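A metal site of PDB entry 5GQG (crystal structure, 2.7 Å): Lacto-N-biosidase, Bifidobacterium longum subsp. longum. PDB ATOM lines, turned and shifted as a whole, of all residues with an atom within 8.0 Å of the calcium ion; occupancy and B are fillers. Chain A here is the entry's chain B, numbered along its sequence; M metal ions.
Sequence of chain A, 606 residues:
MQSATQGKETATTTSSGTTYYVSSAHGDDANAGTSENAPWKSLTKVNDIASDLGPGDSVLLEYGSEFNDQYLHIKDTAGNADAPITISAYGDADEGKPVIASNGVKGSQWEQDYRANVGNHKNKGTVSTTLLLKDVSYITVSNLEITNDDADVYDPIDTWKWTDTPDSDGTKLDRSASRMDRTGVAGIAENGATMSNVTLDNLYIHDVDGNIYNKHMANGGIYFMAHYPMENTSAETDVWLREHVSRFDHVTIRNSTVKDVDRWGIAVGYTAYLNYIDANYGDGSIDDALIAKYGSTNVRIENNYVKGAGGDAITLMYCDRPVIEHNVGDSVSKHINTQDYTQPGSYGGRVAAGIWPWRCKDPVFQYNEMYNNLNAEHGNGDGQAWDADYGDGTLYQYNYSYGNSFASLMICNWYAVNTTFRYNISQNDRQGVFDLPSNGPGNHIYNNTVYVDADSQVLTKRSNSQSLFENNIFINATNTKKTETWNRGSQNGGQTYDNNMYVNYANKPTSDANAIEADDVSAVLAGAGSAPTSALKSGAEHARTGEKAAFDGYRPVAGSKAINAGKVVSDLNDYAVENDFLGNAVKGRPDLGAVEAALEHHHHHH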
ATOM      1  N   ASN A 148      23.162  35.272  20.450  1.00  0.00           N
ATOM      2  CA  ASN A 148      24.356  34.811  21.155  1.00  0.00           C
ATOM      3  C   ASN A 148      24.798  33.457  20.573  1.00  0.00           C
ATOM      4  O   ASN A 148      24.790  32.412  21.229  1.00  0.00           O
ATOM      5  CB  ASN A 148      24.140  34.790  22.676  1.00  0.00           C
ATOM      6  CG  ASN A 148      25.457  34.909  23.432  1.00  0.00           C
ATOM      7  OD1 ASN A 148      26.483  34.388  22.989  1.00  0.00           O
ATOM      8  ND2 ASN A 148      25.436  35.615  24.565  1.00  0.00           N
ATOM      9  N   ASP A 149      25.202  33.519  19.320  1.00  0.00           N
ATOM     10  CA  ASP A 149      25.447  32.333  18.499  1.00  0.00           C
ATOM     11  C   ASP A 149      26.813  31.690  18.777  1.00  0.00           C
ATOM     12  O   ASP A 149      27.746  32.365  19.153  1.00  0.00           O
ATOM     13  CB  ASP A 149      25.305  32.697  17.009  1.00  0.00           C
ATOM     14  CG  ASP A 149      25.609  31.545  16.099  1.00  0.00           C
ATOM     15  OD1 ASP A 149      24.743  30.675  15.921  1.00  0.00           O
ATOM     16  OD2 ASP A 149      26.733  31.496  15.590  1.00  0.00           O
ATOM     17  N   ASP A 150      26.877  30.378  18.624  1.00  0.00           N
ATOM     18  CA  ASP A 150      28.111  29.621  18.593  1.00  0.00           C
ATOM     19  C   ASP A 150      28.072  28.965  17.224  1.00  0.00           C
ATOM     20  O   ASP A 150      27.068  28.324  16.855  1.00  0.00           O
ATOM     21  CB  ASP A 150      28.125  28.597  19.722  1.00  0.00           C
ATOM     22  CG  ASP A 150      29.358  27.711  19.739  1.00  0.00           C
ATOM     23  OD1 ASP A 150      30.149  27.633  18.769  1.00  0.00           O
ATOM     24  OD2 ASP A 150      29.517  27.044  20.777  1.00  0.00           O
ATOM     25  N   ALA A 151      29.152  29.171  16.470  1.00  0.00           N
ATOM     26  CA  ALA A 151      29.263  28.672  15.108  1.00  0.00           C
ATOM     27  C   ALA A 151      29.367  27.146  15.067  1.00  0.00           C
ATOM     28  O   ALA A 151      29.061  26.511  14.052  1.00  0.00           O
ATOM     29  CB  ALA A 151      30.451  29.302  14.425  1.00  0.00           C
ATOM     30  N   ASP A 152      29.807  26.559  16.172  1.00  0.00           N
ATOM     31  CA  ASP A 152      29.919  25.111  16.311  1.00  0.00           C
ATOM     32  C   ASP A 152      28.606  24.460  16.809  1.00  0.00           C
ATOM     33  O   ASP A 152      28.612  23.261  17.058  1.00  0.00           O
ATOM     34  CB  ASP A 152      31.051  24.789  17.304  1.00  0.00           C
ATOM     35  CG  ASP A 152      32.115  23.902  16.713  1.00  0.00           C
ATOM     36  OD1 ASP A 152      31.836  23.055  15.828  1.00  0.00           O
ATOM     37  OD2 ASP A 152      33.271  24.079  17.169  1.00  0.00           O
ATOM     38  N   VAL A 153      27.530  25.231  16.999  1.00  0.00           N
ATOM     39  CA  VAL A 153      26.192  24.703  17.275  1.00  0.00           C
ATOM     40  C   VAL A 153      25.209  25.152  16.205  1.00  0.00           C
ATOM     41  O   VAL A 153      25.149  26.328  15.883  1.00  0.00           O
ATOM     42  CB  VAL A 153      25.646  25.198  18.626  1.00  0.00           C
ATOM     43  CG1 VAL A 153      24.194  24.763  18.836  1.00  0.00           C
ATOM     44  CG2 VAL A 153      26.521  24.712  19.763  1.00  0.00           C
ATOM     45  N   TYR A 154      24.397  24.218  15.702  1.00  0.00           N
ATOM     46  CA  TYR A 154      23.460  24.505  14.634  1.00  0.00           C
ATOM     47  C   TYR A 154      22.377  23.430  14.540  1.00  0.00           C
ATOM     48  O   TYR A 154      22.659  22.265  14.235  1.00  0.00           O
ATOM     49  CB  TYR A 154      24.220  24.590  13.310  1.00  0.00           C
ATOM     50  CG  TYR A 154      23.346  24.956  12.150  1.00  0.00           C
ATOM     51  CD1 TYR A 154      22.691  26.186  12.103  1.00  0.00           C
ATOM     52  CD2 TYR A 154      23.170  24.080  11.083  1.00  0.00           C
ATOM     53  CE1 TYR A 154      21.877  26.515  11.032  1.00  0.00           C
ATOM     54  CE2 TYR A 154      22.364  24.411  10.006  1.00  0.00           C
ATOM     55  CZ  TYR A 154      21.716  25.630   9.987  1.00  0.00           C
ATOM     56  OH  TYR A 154      20.930  25.949   8.919  1.00  0.00           O
ATOM     57  N   ASP A 155      21.140  23.806  14.826  1.00  0.00           N
ATOM     58  CA  ASP A 155      20.042  22.864  14.831  1.00  0.00           C
ATOM     59  C   ASP A 155      18.749  23.660  14.720  1.00  0.00           C
ATOM     60  O   ASP A 155      17.952  23.664  15.645  1.00  0.00           O
ATOM     61  CB  ASP A 155      20.077  22.013  16.106  1.00  0.00           C
ATOM     62  CG  ASP A 155      19.119  20.794  16.048  1.00  0.00           C
ATOM     63  OD1 ASP A 155      18.535  20.466  14.977  1.00  0.00           O
ATOM     64  OD2 ASP A 155      19.002  20.153  17.124  1.00  0.00           O
ATOM     65  N   PRO A 156      18.540  24.342  13.586  1.00  0.00           N
ATOM     66  CA  PRO A 156      17.411  25.213  13.392  1.00  0.00           C
ATOM     67  C   PRO A 156      16.067  24.502  13.507  1.00  0.00           C
ATOM     68  O   PRO A 156      15.917  23.366  13.031  1.00  0.00           O
ATOM     69  CB  PRO A 156      17.578  25.688  11.962  1.00  0.00           C
ATOM     70  CG  PRO A 156      18.307  24.577  11.302  1.00  0.00           C
ATOM     71  CD  PRO A 156      19.319  24.218  12.343  1.00  0.00           C
ATOM     72  N   LYS A 172      24.637  20.058  14.516  1.00  0.00           N
ATOM     73  CA  LYS A 172      25.657  19.784  15.569  1.00  0.00           C
ATOM     74  C   LYS A 172      25.317  20.502  16.897  1.00  0.00           C
ATOM     75  O   LYS A 172      24.949  21.691  16.918  1.00  0.00           O
ATOM     76  CB  LYS A 172      27.123  20.101  15.111  1.00  0.00           C
ATOM     77  CG  LYS A 172      27.332  21.510  14.547  1.00  0.00           C
ATOM     78  CD  LYS A 172      28.357  21.622  13.404  1.00  0.00           C
ATOM     79  CE  LYS A 172      27.799  22.372  12.184  1.00  0.00           C
ATOM     80  NZ  LYS A 172      28.527  22.045  10.931  1.00  0.00           N
ATOM     81  N   LEU A 173      25.448  19.753  17.985  1.00  0.00           N
ATOM     82  CA  LEU A 173      25.104  20.251  19.299  1.00  0.00           C
ATOM     83  C   LEU A 173      26.237  20.088  20.328  1.00  0.00           C
ATOM     84  O   LEU A 173      27.031  19.176  20.246  1.00  0.00           O
ATOM     85  CB  LEU A 173      23.850  19.489  19.774  1.00  0.00           C
ATOM     86  CG  LEU A 173      22.505  19.837  19.127  1.00  0.00           C
ATOM     87  CD1 LEU A 173      21.424  18.916  19.673  1.00  0.00           C
ATOM     88  CD2 LEU A 173      22.082  21.279  19.343  1.00  0.00           C
ATOM     89  N   ARG A 179      28.450  23.153  29.728  1.00  0.00           N
ATOM     90  CA  ARG A 179      28.487  24.175  28.699  1.00  0.00           C
ATOM     91  C   ARG A 179      28.154  25.522  29.338  1.00  0.00           C
ATOM     92  O   ARG A 179      27.333  25.618  30.263  1.00  0.00           O
ATOM     93  CB  ARG A 179      27.564  23.831  27.519  1.00  0.00           C
ATOM     94  CG  ARG A 179      27.532  24.890  26.444  1.00  0.00           C
ATOM     95  CD  ARG A 179      26.600  24.519  25.322  1.00  0.00           C
ATOM     96  NE  ARG A 179      26.475  25.611  24.370  1.00  0.00           N
ATOM     97  CZ  ARG A 179      27.374  25.955  23.434  1.00  0.00           C
ATOM     98  NH1 ARG A 179      28.511  25.272  23.302  1.00  0.00           N
ATOM     99  NH2 ARG A 179      27.125  26.977  22.629  1.00  0.00           N
ATOM    100  N   ARG A 182      24.187  30.742  28.380  1.00  0.00           N
ATOM    101  CA  ARG A 182      24.053  31.986  27.577  1.00  0.00           C
ATOM    102  C   ARG A 182      22.658  32.643  27.614  1.00  0.00           C
ATOM    103  O   ARG A 182      21.642  31.959  27.633  1.00  0.00           O
ATOM    104  CB  ARG A 182      24.379  31.708  26.111  1.00  0.00           C
ATOM    105  CG  ARG A 182      25.736  31.074  25.866  1.00  0.00           C
ATOM    106  CD  ARG A 182      26.223  31.335  24.429  1.00  0.00           C
ATOM    107  NE  ARG A 182      27.474  30.631  24.155  1.00  0.00           N
ATOM    108  CZ  ARG A 182      28.203  30.740  23.050  1.00  0.00           C
ATOM    109  NH1 ARG A 182      27.837  31.525  22.048  1.00  0.00           N
ATOM    110  NH2 ARG A 182      29.319  30.022  22.935  1.00  0.00           N
ATOM    111  N   HIS A 206      17.382  35.576  18.815  1.00  0.00           N
ATOM    112  CA  HIS A 206      17.580  34.239  18.245  1.00  0.00           C
ATOM    113  C   HIS A 206      19.014  33.738  18.227  1.00  0.00           C
ATOM    114  O   HIS A 206      19.975  34.489  18.418  1.00  0.00           O
ATOM    115  CB  HIS A 206      16.966  34.136  16.834  1.00  0.00           C
ATOM    116  CG  HIS A 206      17.729  34.884  15.785  1.00  0.00           C
ATOM    117  ND1 HIS A 206      18.668  34.279  14.979  1.00  0.00           N
ATOM    118  CD2 HIS A 206      17.723  36.196  15.446  1.00  0.00           C
ATOM    119  CE1 HIS A 206      19.191  35.183  14.167  1.00  0.00           C
ATOM    120  NE2 HIS A 206      18.648  36.354  14.436  1.00  0.00           N
ATOM    121  N   ASP A 207      19.130  32.430  18.005  1.00  0.00           N
ATOM    122  CA  ASP A 207      20.401  31.725  17.988  1.00  0.00           C
ATOM    123  C   ASP A 207      21.226  32.041  19.251  1.00  0.00           C
ATOM    124  O   ASP A 207      22.343  32.567  19.189  1.00  0.00           O
ATOM    125  CB  ASP A 207      21.145  32.002  16.679  1.00  0.00           C
ATOM    126  CG  ASP A 207      20.493  31.318  15.501  1.00  0.00           C
ATOM    127  OD1 ASP A 207      19.591  31.895  14.888  1.00  0.00           O
ATOM    128  OD2 ASP A 207      20.874  30.191  15.171  1.00  0.00           O
ATOM    129  N   VAL A 208      20.611  31.755  20.404  1.00  0.00           N
ATOM    130  CA  VAL A 208      21.268  31.859  21.714  1.00  0.00           C
ATOM    131  C   VAL A 208      21.592  30.415  22.116  1.00  0.00           C
ATOM    132  O   VAL A 208      20.790  29.737  22.777  1.00  0.00           O
ATOM    133  CB  VAL A 208      20.358  32.566  22.740  1.00  0.00           C
ATOM    134  CG1 VAL A 208      20.998  32.596  24.139  1.00  0.00           C
ATOM    135  CG2 VAL A 208      20.003  33.972  22.262  1.00  0.00           C
ATOM    136  N   ASP A 209      22.771  29.954  21.719  1.00  0.00           N
ATOM    137  CA  ASP A 209      23.174  28.568  21.956  1.00  0.00           C
ATOM    138  C   ASP A 209      23.654  28.393  23.381  1.00  0.00           C
ATOM    139  O   ASP A 209      24.836  28.148  23.639  1.00  0.00           O
ATOM    140  CB  ASP A 209      24.248  28.141  20.948  1.00  0.00           C
ATOM    141  CG  ASP A 209      23.806  28.339  19.515  1.00  0.00           C
ATOM    142  OD1 ASP A 209      22.606  28.380  19.241  1.00  0.00           O
ATOM    143  OD2 ASP A 209      24.685  28.470  18.634  1.00  0.00           O
ATOM    144  N   ASP A 260      15.062  29.650  18.273  1.00  0.00           N
ATOM    145  CA  ASP A 260      16.312  28.887  18.211  1.00  0.00           C
ATOM    146  C   ASP A 260      17.231  29.187  19.430  1.00  0.00           C
ATOM    147  O   ASP A 260      18.406  29.533  19.309  1.00  0.00           O
ATOM    148  CB  ASP A 260      17.019  29.104  16.867  1.00  0.00           C
ATOM    149  CG  ASP A 260      16.550  28.108  15.763  1.00  0.00           C
ATOM    150  OD1 ASP A 260      16.142  26.972  16.067  1.00  0.00           O
ATOM    151  OD2 ASP A 260      16.637  28.444  14.556  1.00  0.00           O
HETATM  152 CA    CA M   1      23.735  28.394  16.298  1.00  0.00          CA
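OD2 of Asp 150 lies within salt-bridge range of NH2 of Arg 179 (3.0 Å). The guanidinium group of Arg 182 lies within salt-bridge range of the side-chain carboxylate of Asp 150, 3.7 Å away. The guanidinium group of Arg 182 sits at hydrogen-bond distance from the backbone carbonyl oxygen of Asp 149 (3.0 Å). OD2 of Asp 149 lies within hydrogen-bond range of N of Ala 151 (3.5 Å). A ring nitrogen (ND1) of His 206 lies within hydrogen-bond range of the side-chain carboxylate of Asp 207, at 2.6 Å. The backbone NH of Asp 149 sits at hydrogen-bond distance from the backbone carbonyl oxygen of Asp 207, 3.0 Å away. The backbone carbonyl oxygen (O) of Asp 207 sits close to the backbone NH (N) of Asn 148 (3.1 Å). The backbone NH (N) of Asp 150 lies close to the side-chain carboxylate (OD2) of Asp 209.
O of Asp 150 touches the calcium ion (3.4 Å). Asp 207 touches the calcium ion (OD2 to CA, 3.6 Å). Within 4 Å of the calcium ion: Asp 149, Asp 150, Val 153, Asp 207 and Asp 209.
The calcium ion is bound by OD1 of Asp 149, OD2 of Asp 209 and O of Val 153. The calcium ion has three donor atoms within binding distance.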
